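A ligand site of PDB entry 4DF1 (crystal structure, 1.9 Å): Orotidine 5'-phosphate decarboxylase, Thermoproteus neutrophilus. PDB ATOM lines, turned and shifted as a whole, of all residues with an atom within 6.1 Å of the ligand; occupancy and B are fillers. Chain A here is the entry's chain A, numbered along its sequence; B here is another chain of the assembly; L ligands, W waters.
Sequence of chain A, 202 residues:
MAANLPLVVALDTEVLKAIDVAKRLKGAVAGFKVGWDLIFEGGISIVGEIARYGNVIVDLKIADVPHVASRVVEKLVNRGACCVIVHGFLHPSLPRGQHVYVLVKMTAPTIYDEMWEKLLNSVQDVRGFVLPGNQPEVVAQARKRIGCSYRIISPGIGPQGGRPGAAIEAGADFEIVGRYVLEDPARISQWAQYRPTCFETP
An oxygen (O9) of the ligand is in hydrogen-bond range of the backbone NH (N) of Thr 107 (2.9 Å).
NE of Arg 179 is in salt-bridge range of O2 of the ligand (2.8 Å).
NZ of Lys 61 sits at hydrogen-bond distance from O10 of the ligand (2.8 Å).
OD2 of Asp 59 sits at hydrogen-bond distance from O10 of the ligand (3.3 Å).
An oxygen (O3) of the ligand lies within hydrogen-bond range of the backbone NH of Gly 178, at 2.8 Å.
The backbone NH (N) of Arg 179 lies within hydrogen-bond range of an oxygen (O2) of the ligand, 2.8 Å away.
N2 of the ligand sits at hydrogen-bond distance from OG1 of Thr 107 (2.8 Å).
The side-chain amino group of Lys 33 is in hydrogen-bond range of an oxygen (O6) of the ligand (2.7 Å).
The side-chain carboxylate of Asp 12 is in hydrogen-bond range of an oxygen (O6) of the ligand (2.6 Å).
OD1 of Asp 64 of chain B lies within hydrogen-bond range of O7 of the ligand, 2.7 Å away.
O8 of the ligand sits at hydrogen-bond distance from NE2 of Gln 160, 2.9 Å away.
Residues that only touch the ligand: Ala 10 (3.97 Å), Met 106 (3.2 Å), Pro 155 (3.3 Å), Ile 157 (3.8 Å), Ile 176 (3.99 Å), Val 177 (3.8 Å), Val 65 of chain B (3.5 Å), His 67 of chain B (3.6 Å) and Val 68 of chain B (3.7 Å).
Hydrophobic or aromatic side chains that line the ligand: Ala 10, Met 106, Pro 155, Ile 176, Val 65 of chain B, His 67 of chain B and Val 68 of chain B.
18 residues have an atom within 4 Å of the ligand: Ala 10, Asp 12, Lys 33, Asp 59, Lys 61, Met 106, Thr 107, Pro 155, Ile 157, Gln 160, Ile 176, Val 177, Gly 178, Arg 179, Asp 64 of chain B, Val 65 of chain B, His 67 of chain B and Val 68 of chain B.
The nearest printed residue that does not touch the ligand is Leu 103 (4.1 Å).
The side-chain carboxylate (OD2) of Asp 64 of chain B is in salt-bridge range of the side-chain amino group (NZ) of Lys 61 (2.8 Å).
NH2 of Arg 179 lies close to NE2 of His 67 of chain B (3.4 Å).
The side-chain amino group of Lys 33 is in salt-bridge range of the side-chain carboxylate of Asp 59 (2.7 Å).
The backbone carbonyl oxygen of Val 177 sits at hydrogen-bond distance from the backbone NH of Ala 10 (2.8 Å).
The side-chain hydroxyl (OG1) of Thr 107 is in hydrogen-bond range of the side-chain amide oxygen (OE1) of Gln 160, at 2.6 Å.
The side-chain carboxylate (OD2) of Asp 59 lies within salt-bridge range of the side-chain amino group (NZ) of Lys 61.
Water W5 lies within hydrogen-bond range of an oxygen (O3) of the ligand (2.6 Å), the backbone carbonyl oxygen of Ile 157 (2.8 Å), the backbone NH of Tyr 180 (2.9 Å) and the backbone NH of Arg 179 (3.4 Å).
Water W1 lies within hydrogen-bond range of O3 of the ligand (2.6 Å), O of Ile 176 (2.6 Å), N of Gly 156 (2.8 Å) and N of Ile 157 (2.9 Å).
Water W2 lies within hydrogen-bond range of the side-chain carboxylate of Asp 12 (2.6 Å), an oxygen (O2) of the ligand (2.7 Å) and a ring nitrogen (NE2) of His 67 of chain B (3.0 Å).
Water W4 lies within hydrogen-bond range of O1 of the ligand (2.8 Å), O of Ile 157 (2.8 Å) and N of Gln 160 (2.9 Å).
Water W3 lies within hydrogen-bond range of an oxygen (O7) of the ligand (2.9 Å), the side-chain carboxylate (OD1) of Asp 12 (3.2 Å), the side-chain carboxylate (OD2) of Asp 64 of chain B (3.3 Å) and the side-chain amino group (NZ) of Lys 33 (3.4 Å).
Water W6 lies within hydrogen-bond range of the backbone carbonyl oxygen (O) of Lys 105 (2.9 Å) and an oxygen (O9) of the ligand (3.0 Å).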
ATOM      1  N   ALA A  10      24.925 -23.417 -24.995  1.00  0.00           N
ATOM      2  CA  ALA A  10      23.773 -23.091 -25.842  1.00  0.00           C
ATOM      3  C   ALA A  10      24.086 -23.396 -27.306  1.00  0.00           C
ATOM      4  O   ALA A  10      24.978 -22.777 -27.890  1.00  0.00           O
ATOM      5  CB  ALA A  10      23.415 -21.623 -25.672  1.00  0.00           C
ATOM      6  N   ASP A  12      23.017 -22.756 -30.298  1.00  0.00           N
ATOM      7  CA  ASP A  12      22.240 -21.905 -31.195  1.00  0.00           C
ATOM      8  C   ASP A  12      22.944 -21.957 -32.544  1.00  0.00           C
ATOM      9  O   ASP A  12      23.630 -21.015 -32.956  1.00  0.00           O
ATOM     10  CB  ASP A  12      22.201 -20.465 -30.677  1.00  0.00           C
ATOM     11  CG  ASP A  12      21.533 -20.355 -29.303  1.00  0.00           C
ATOM     12  OD1 ASP A  12      20.474 -20.976 -29.094  1.00  0.00           O
ATOM     13  OD2 ASP A  12      22.070 -19.625 -28.432  1.00  0.00           O
ATOM     14  N   LYS A  33      21.797 -26.516 -24.183  1.00  0.00           N
ATOM     15  CA  LYS A  33      20.542 -25.800 -24.353  1.00  0.00           C
ATOM     16  C   LYS A  33      20.185 -25.847 -25.831  1.00  0.00           C
ATOM     17  O   LYS A  33      20.955 -25.429 -26.690  1.00  0.00           O
ATOM     18  CB  LYS A  33      20.654 -24.347 -23.857  1.00  0.00           C
ATOM     19  CG  LYS A  33      19.288 -23.639 -23.694  1.00  0.00           C
ATOM     20  CD  LYS A  33      19.419 -22.272 -23.036  1.00  0.00           C
ATOM     21  CE  LYS A  33      19.958 -21.198 -23.989  1.00  0.00           C
ATOM     22  NZ  LYS A  33      19.019 -20.930 -25.125  1.00  0.00           N
ATOM     23  N   ASP A  59      14.973 -24.723 -24.830  1.00  0.00           N
ATOM     24  CA  ASP A  59      14.656 -23.325 -24.599  1.00  0.00           C
ATOM     25  C   ASP A  59      13.975 -22.716 -25.802  1.00  0.00           C
ATOM     26  O   ASP A  59      14.640 -22.300 -26.755  1.00  0.00           O
ATOM     27  CB  ASP A  59      15.929 -22.546 -24.265  1.00  0.00           C
ATOM     28  CG  ASP A  59      15.666 -21.076 -24.015  1.00  0.00           C
ATOM     29  OD1 ASP A  59      14.474 -20.706 -23.838  1.00  0.00           O
ATOM     30  OD2 ASP A  59      16.638 -20.298 -23.991  1.00  0.00           O
ATOM     31  N   LYS A  61      11.647 -20.385 -24.928  1.00  0.00           N
ATOM     32  CA  LYS A  61      11.082 -19.238 -24.222  1.00  0.00           C
ATOM     33  C   LYS A  61       9.571 -19.389 -24.154  1.00  0.00           C
ATOM     34  O   LYS A  61       8.823 -18.461 -24.490  1.00  0.00           O
ATOM     35  CB  LYS A  61      11.464 -17.937 -24.945  1.00  0.00           C
ATOM     36  CG  LYS A  61      12.990 -17.645 -24.993  1.00  0.00           C
ATOM     37  CD  LYS A  61      13.584 -17.371 -23.600  1.00  0.00           C
ATOM     38  CE  LYS A  61      15.030 -16.865 -23.701  1.00  0.00           C
ATOM     39  NZ  LYS A  61      15.889 -17.807 -24.490  1.00  0.00           N
ATOM     40  N   ILE A  85      12.679 -24.133 -20.489  1.00  0.00           N
ATOM     41  CA  ILE A  85      12.605 -22.757 -20.004  1.00  0.00           C
ATOM     42  C   ILE A  85      11.283 -22.134 -20.421  1.00  0.00           C
ATOM     43  O   ILE A  85      10.876 -22.266 -21.584  1.00  0.00           O
ATOM     44  CB  ILE A  85      13.804 -21.926 -20.507  1.00  0.00           C
ATOM     45  CG1 ILE A  85      15.094 -22.442 -19.872  1.00  0.00           C
ATOM     46  CG2 ILE A  85      13.592 -20.414 -20.257  1.00  0.00           C
ATOM     47  CD1 ILE A  85      16.341 -21.788 -20.395  1.00  0.00           C
ATOM     48  N   LEU A 103      12.156 -17.963 -16.492  1.00  0.00           N
ATOM     49  CA  LEU A 103      12.919 -16.751 -16.769  1.00  0.00           C
ATOM     50  C   LEU A 103      12.198 -15.572 -16.129  1.00  0.00           C
ATOM     51  O   LEU A 103      11.033 -15.358 -16.403  1.00  0.00           O
ATOM     52  CB  LEU A 103      13.015 -16.563 -18.287  1.00  0.00           C
ATOM     53  CG  LEU A 103      13.716 -15.358 -18.917  1.00  0.00           C
ATOM     54  CD1 LEU A 103      15.138 -15.232 -18.441  1.00  0.00           C
ATOM     55  CD2 LEU A 103      13.701 -15.491 -20.459  1.00  0.00           C
ATOM     56  N   LYS A 105      14.052 -12.299 -15.533  1.00  0.00           N
ATOM     57  CA  LYS A 105      14.696 -11.046 -15.927  1.00  0.00           C
ATOM     58  C   LYS A 105      15.619 -11.422 -17.085  1.00  0.00           C
ATOM     59  O   LYS A 105      16.162 -12.520 -17.102  1.00  0.00           O
ATOM     60  CB  LYS A 105      15.516 -10.444 -14.765  1.00  0.00           C
ATOM     61  CG  LYS A 105      15.909  -8.968 -14.981  1.00  0.00           C
ATOM     62  CD  LYS A 105      16.795  -8.426 -13.850  1.00  0.00           C
ATOM     63  CE  LYS A 105      16.795  -6.883 -13.829  1.00  0.00           C
ATOM     64  NZ  LYS A 105      17.510  -6.297 -14.997  1.00  0.00           N
ATOM     65  N   MET A 106      15.782 -10.534 -18.063  1.00  0.00           N
ATOM     66  CA  MET A 106      16.589 -10.904 -19.221  1.00  0.00           C
ATOM     67  C   MET A 106      17.890 -10.128 -19.316  1.00  0.00           C
ATOM     68  O   MET A 106      18.066  -9.120 -18.638  1.00  0.00           O
ATOM     69  CB  MET A 106      15.761 -10.796 -20.506  1.00  0.00           C
ATOM     70  CG  MET A 106      14.494 -11.662 -20.436  1.00  0.00           C
ATOM     71  SD  MET A 106      13.574 -11.704 -21.980  1.00  0.00           S
ATOM     72  CE  MET A 106      14.650 -12.711 -22.987  1.00  0.00           C
ATOM     73  N   THR A 107      18.795 -10.594 -20.175  1.00  0.00           N
ATOM     74  CA  THR A 107      20.097  -9.953 -20.383  1.00  0.00           C
ATOM     75  C   THR A 107      19.929  -8.702 -21.242  1.00  0.00           C
ATOM     76  O   THR A 107      20.874  -7.920 -21.379  1.00  0.00           O
ATOM     77  CB  THR A 107      21.090 -10.915 -21.068  1.00  0.00           C
ATOM     78  OG1 THR A 107      20.478 -11.444 -22.264  1.00  0.00           O
ATOM     79  CG2 THR A 107      21.445 -12.081 -20.127  1.00  0.00           C
ATOM     80  N   ALA A 108      18.749  -8.546 -21.819  1.00  0.00           N
ATOM     81  CA  ALA A 108      18.365  -7.328 -22.561  1.00  0.00           C
ATOM     82  C   ALA A 108      17.228  -6.628 -21.786  1.00  0.00           C
ATOM     83  O   ALA A 108      16.496  -7.280 -21.044  1.00  0.00           O
ATOM     84  CB  ALA A 108      17.898  -7.691 -23.977  1.00  0.00           C
ATOM     85  N   VAL A 130      15.903 -18.456 -14.384  1.00  0.00           N
ATOM     86  CA  VAL A 130      16.916 -17.945 -15.299  1.00  0.00           C
ATOM     87  C   VAL A 130      17.078 -16.467 -14.967  1.00  0.00           C
ATOM     88  O   VAL A 130      16.094 -15.702 -14.999  1.00  0.00           O
ATOM     89  CB  VAL A 130      16.531 -18.124 -16.781  1.00  0.00           C
ATOM     90  CG1 VAL A 130      17.678 -17.687 -17.703  1.00  0.00           C
ATOM     91  CG2 VAL A 130      16.160 -19.588 -17.070  1.00  0.00           C
ATOM     92  N   PRO A 132      19.917 -12.979 -15.404  1.00  0.00           N
ATOM     93  CA  PRO A 132      20.944 -12.525 -16.361  1.00  0.00           C
ATOM     94  C   PRO A 132      22.364 -12.534 -15.805  1.00  0.00           C
ATOM     95  O   PRO A 132      22.648 -11.816 -14.842  1.00  0.00           O
ATOM     96  CB  PRO A 132      20.496 -11.096 -16.716  1.00  0.00           C
ATOM     97  CG  PRO A 132      19.609 -10.659 -15.562  1.00  0.00           C
ATOM     98  CD  PRO A 132      18.933 -11.937 -15.075  1.00  0.00           C
ATOM     99  N   PRO A 155      22.531 -16.796 -18.488  1.00  0.00           N
ATOM    100  CA  PRO A 155      23.168 -16.512 -19.779  1.00  0.00           C
ATOM    101  C   PRO A 155      23.773 -15.110 -19.823  1.00  0.00           C
ATOM    102  O   PRO A 155      23.710 -14.369 -18.837  1.00  0.00           O
ATOM    103  CB  PRO A 155      21.979 -16.565 -20.746  1.00  0.00           C
ATOM    104  CG  PRO A 155      20.853 -15.976 -19.932  1.00  0.00           C
ATOM    105  CD  PRO A 155      21.091 -16.492 -18.509  1.00  0.00           C
ATOM    106  N   GLY A 156      24.356 -14.761 -20.969  1.00  0.00           N
ATOM    107  CA  GLY A 156      24.869 -13.419 -21.162  1.00  0.00           C
ATOM    108  C   GLY A 156      26.365 -13.298 -20.990  1.00  0.00           C
ATOM    109  O   GLY A 156      26.899 -12.208 -20.725  1.00  0.00           O
ATOM    110  N   ILE A 157      27.074 -14.410 -21.146  1.00  0.00           N
ATOM    111  CA  ILE A 157      28.520 -14.408 -20.954  1.00  0.00           C
ATOM    112  C   ILE A 157      29.209 -14.249 -22.317  1.00  0.00           C
ATOM    113  O   ILE A 157      28.875 -14.937 -23.275  1.00  0.00           O
ATOM    114  CB  ILE A 157      28.982 -15.734 -20.305  1.00  0.00           C
ATOM    115  CG1 ILE A 157      28.189 -16.017 -19.004  1.00  0.00           C
ATOM    116  CG2 ILE A 157      30.501 -15.735 -20.110  1.00  0.00           C
ATOM    117  CD1 ILE A 157      28.247 -14.910 -17.976  1.00  0.00           C
ATOM    118  N   GLY A 158      30.171 -13.331 -22.393  1.00  0.00           N
ATOM    119  CA  GLY A 158      30.915 -13.128 -23.627  1.00  0.00           C
ATOM    120  C   GLY A 158      30.377 -11.914 -24.368  1.00  0.00           C
ATOM    121  O   GLY A 158      30.399 -10.813 -23.829  1.00  0.00           O
ATOM    122  N   PRO A 159      29.882 -12.114 -25.596  1.00  0.00           N
ATOM    123  CA  PRO A 159      29.352 -11.016 -26.413  1.00  0.00           C
ATOM    124  C   PRO A 159      28.372 -10.092 -25.682  1.00  0.00           C
ATOM    125  O   PRO A 159      28.400  -8.875 -25.901  1.00  0.00           O
ATOM    126  CB  PRO A 159      28.640 -11.746 -27.558  1.00  0.00           C
ATOM    127  CG  PRO A 159      29.428 -12.998 -27.718  1.00  0.00           C
ATOM    128  CD  PRO A 159      29.834 -13.409 -26.308  1.00  0.00           C
ATOM    129  N   GLN A 160      27.522 -10.642 -24.824  1.00  0.00           N
ATOM    130  CA  GLN A 160      26.554  -9.807 -24.124  1.00  0.00           C
ATOM    131  C   GLN A 160      27.133  -9.112 -22.910  1.00  0.00           C
ATOM    132  O   GLN A 160      26.427  -8.369 -22.220  1.00  0.00           O
ATOM    133  CB  GLN A 160      25.310 -10.600 -23.735  1.00  0.00           C
ATOM    134  CG  GLN A 160      24.544 -11.140 -24.937  1.00  0.00           C
ATOM    135  CD  GLN A 160      23.240 -11.747 -24.513  1.00  0.00           C
ATOM    136  OE1 GLN A 160      22.330 -11.045 -24.071  1.00  0.00           O
ATOM    137  NE2 GLN A 160      23.146 -13.068 -24.634  1.00  0.00           N
ATOM    138  N   ILE A 176      25.067 -20.211 -18.782  1.00  0.00           N
ATOM    139  CA  ILE A 176      24.629 -20.635 -20.106  1.00  0.00           C
ATOM    140  C   ILE A 176      25.463 -19.853 -21.112  1.00  0.00           C
ATOM    141  O   ILE A 176      25.462 -18.617 -21.107  1.00  0.00           O
ATOM    142  CB  ILE A 176      23.162 -20.294 -20.328  1.00  0.00           C
ATOM    143  CG1 ILE A 176      22.270 -21.094 -19.370  1.00  0.00           C
ATOM    144  CG2 ILE A 176      22.755 -20.577 -21.783  1.00  0.00           C
ATOM    145  CD1 ILE A 176      20.859 -20.534 -19.240  1.00  0.00           C
ATOM    146  N   VAL A 177      26.196 -20.564 -21.964  1.00  0.00           N
ATOM    147  CA  VAL A 177      27.137 -19.897 -22.859  1.00  0.00           C
ATOM    148  C   VAL A 177      27.014 -20.463 -24.272  1.00  0.00           C
ATOM    149  O   VAL A 177      27.094 -21.670 -24.479  1.00  0.00           O
ATOM    150  CB  VAL A 177      28.599 -20.071 -22.372  1.00  0.00           C
ATOM    151  CG1 VAL A 177      29.517 -19.240 -23.221  1.00  0.00           C
ATOM    152  CG2 VAL A 177      28.726 -19.667 -20.881  1.00  0.00           C
ATOM    153  N   GLY A 178      26.833 -19.564 -25.243  1.00  0.00           N
ATOM    154  CA  GLY A 178      26.629 -19.979 -26.622  1.00  0.00           C
ATOM    155  C   GLY A 178      27.816 -19.646 -27.507  1.00  0.00           C
ATOM    156  O   GLY A 178      28.777 -20.418 -27.603  1.00  0.00           O
ATOM    157  N   ARG A 179      27.759 -18.473 -28.131  1.00  0.00           N
ATOM    158  CA  ARG A 179      28.732 -18.099 -29.163  1.00  0.00           C
ATOM    159  C   ARG A 179      30.189 -18.219 -28.706  1.00  0.00           C
ATOM    160  O   ARG A 179      31.051 -18.664 -29.462  1.00  0.00           O
ATOM    161  CB  ARG A 179      28.456 -16.669 -29.643  1.00  0.00           C
ATOM    162  CG  ARG A 179      27.223 -16.549 -30.547  1.00  0.00           C
ATOM    163  CD  ARG A 179      26.802 -15.087 -30.731  1.00  0.00           C
ATOM    164  NE  ARG A 179      26.199 -14.544 -29.518  1.00  0.00           N
ATOM    165  CZ  ARG A 179      25.790 -13.278 -29.380  1.00  0.00           C
ATOM    166  NH1 ARG A 179      25.929 -12.415 -30.379  1.00  0.00           N
ATOM    167  NH2 ARG A 179      25.247 -12.887 -28.242  1.00  0.00           N
ATOM    168  N   TYR A 180      30.461 -17.806 -27.480  1.00  0.00           N
ATOM    169  CA  TYR A 180      31.834 -17.805 -26.992  1.00  0.00           C
ATOM    170  C   TYR A 180      32.413 -19.225 -27.006  1.00  0.00           C
ATOM    171  O   TYR A 180      33.544 -19.441 -27.457  1.00  0.00           O
ATOM    172  CB  TYR A 180      31.891 -17.189 -25.591  1.00  0.00           C
ATOM    173  CG  TYR A 180      33.283 -16.979 -25.020  1.00  0.00           C
ATOM    174  CD1 TYR A 180      34.165 -16.049 -25.580  1.00  0.00           C
ATOM    175  CD2 TYR A 180      33.707 -17.683 -23.903  1.00  0.00           C
ATOM    176  CE1 TYR A 180      35.435 -15.853 -25.046  1.00  0.00           C
ATOM    177  CE2 TYR A 180      34.966 -17.483 -23.361  1.00  0.00           C
ATOM    178  CZ  TYR A 180      35.832 -16.577 -23.944  1.00  0.00           C
ATOM    179  OH  TYR A 180      37.091 -16.376 -23.415  1.00  0.00           O
ATOM    180  N   ASP B  64      12.693 -13.783 -27.258  1.00  0.00           N
ATOM    181  CA  ASP B  64      14.100 -13.966 -26.954  1.00  0.00           C
ATOM    182  C   ASP B  64      14.813 -12.625 -27.059  1.00  0.00           C
ATOM    183  O   ASP B  64      14.219 -11.629 -27.497  1.00  0.00           O
ATOM    184  CB  ASP B  64      14.713 -15.015 -27.895  1.00  0.00           C
ATOM    185  CG  ASP B  64      15.764 -15.872 -27.214  1.00  0.00           C
ATOM    186  OD1 ASP B  64      16.718 -15.302 -26.632  1.00  0.00           O
ATOM    187  OD2 ASP B  64      15.625 -17.128 -27.241  1.00  0.00           O
ATOM    188  N   VAL B  65      16.074 -12.606 -26.669  1.00  0.00           N
ATOM    189  CA  VAL B  65      16.887 -11.406 -26.787  1.00  0.00           C
ATOM    190  C   VAL B  65      17.200 -11.135 -28.267  1.00  0.00           C
ATOM    191  O   VAL B  65      17.071 -12.031 -29.114  1.00  0.00           O
ATOM    192  CB  VAL B  65      18.184 -11.502 -25.941  1.00  0.00           C
ATOM    193  CG1 VAL B  65      17.839 -11.613 -24.451  1.00  0.00           C
ATOM    194  CG2 VAL B  65      19.055 -12.676 -26.404  1.00  0.00           C
ATOM    195  N   HIS B  67      19.696 -10.790 -30.494  1.00  0.00           N
ATOM    196  CA  HIS B  67      20.527 -11.568 -31.430  1.00  0.00           C
ATOM    197  C   HIS B  67      19.858 -12.872 -31.886  1.00  0.00           C
ATOM    198  O   HIS B  67      20.091 -13.340 -33.005  1.00  0.00           O
ATOM    199  CB  HIS B  67      21.952 -11.794 -30.895  1.00  0.00           C
ATOM    200  CG  HIS B  67      22.097 -12.944 -29.940  1.00  0.00           C
ATOM    201  ND1 HIS B  67      21.854 -12.836 -28.592  1.00  0.00           N
ATOM    202  CD2 HIS B  67      22.564 -14.204 -30.139  1.00  0.00           C
ATOM    203  CE1 HIS B  67      22.113 -13.995 -28.007  1.00  0.00           C
ATOM    204  NE2 HIS B  67      22.559 -14.842 -28.919  1.00  0.00           N
ATOM    205  N   VAL B  68      19.013 -13.441 -31.036  1.00  0.00           N
ATOM    206  CA  VAL B  68      18.280 -14.648 -31.401  1.00  0.00           C
ATOM    207  C   VAL B  68      16.950 -14.294 -32.057  1.00  0.00           C
ATOM    208  O   VAL B  68      16.601 -14.859 -33.101  1.00  0.00           O
ATOM    209  CB  VAL B  68      18.027 -15.558 -30.178  1.00  0.00           C
ATOM    210  CG1 VAL B  68      17.109 -16.738 -30.558  1.00  0.00           C
ATOM    211  CG2 VAL B  68      19.362 -16.062 -29.608  1.00  0.00           C
HETATM  212  P1  LIG L   1      25.228 -16.228 -26.250  1.00  0.00           P
HETATM  213  O1  LIG L   1      25.056 -14.756 -26.063  1.00  0.00           O
HETATM  214  O2  LIG L   1      25.703 -16.597 -27.737  1.00  0.00           O
HETATM  215  O3  LIG L   1      26.188 -16.847 -25.142  1.00  0.00           O
HETATM  216  O4  LIG L   1      23.803 -16.926 -26.147  1.00  0.00           O
HETATM  217  C1  LIG L   1      22.979 -16.727 -25.012  1.00  0.00           C
HETATM  218  C2  LIG L   1      21.877 -17.747 -24.960  1.00  0.00           C
HETATM  219  O5  LIG L   1      21.094 -17.537 -23.762  1.00  0.00           O
HETATM  220  C3  LIG L   1      20.916 -17.709 -26.137  1.00  0.00           C
HETATM  221  O6  LIG L   1      20.497 -19.037 -26.439  1.00  0.00           O
HETATM  222  C4  LIG L   1      19.731 -16.899 -25.598  1.00  0.00           C
HETATM  223  O7  LIG L   1      18.496 -17.233 -26.197  1.00  0.00           O
HETATM  224  C5  LIG L   1      19.752 -17.252 -24.096  1.00  0.00           C
HETATM  225  N1  LIG L   1      19.303 -16.167 -23.218  1.00  0.00           N
HETATM  226  C6  LIG L   1      19.863 -14.938 -23.211  1.00  0.00           C
HETATM  227  O8  LIG L   1      20.800 -14.659 -23.944  1.00  0.00           O
HETATM  228  N2  LIG L   1      19.403 -13.974 -22.394  1.00  0.00           N
HETATM  229  C7  LIG L   1      18.373 -14.202 -21.551  1.00  0.00           C
HETATM  230  O9  LIG L   1      17.979 -13.300 -20.814  1.00  0.00           O
HETATM  231  C8  LIG L   1      17.751 -15.466 -21.529  1.00  0.00           C
HETATM  232  C9  LIG L   1      18.242 -16.433 -22.376  1.00  0.00           C
HETATM  233  O10 LIG L   1      17.713 -17.666 -22.414  1.00  0.00           O
HETATM  234  O   HOH W   1      25.734 -16.469 -22.631  1.00  0.00           O
HETATM  235  O   HOH W   2      23.650 -17.657 -29.183  1.00  0.00           O
HETATM  236  O   HOH W   3      17.876 -19.497 -27.958  1.00  0.00           O
HETATM  237  O   HOH W   4      26.839 -13.438 -24.405  1.00  0.00           O
HETATM  238  O   HOH W   5      28.702 -16.539 -25.553  1.00  0.00           O
HETATM  239  O   HOH W   6      18.518 -13.947 -17.962  1.00  0.00           O
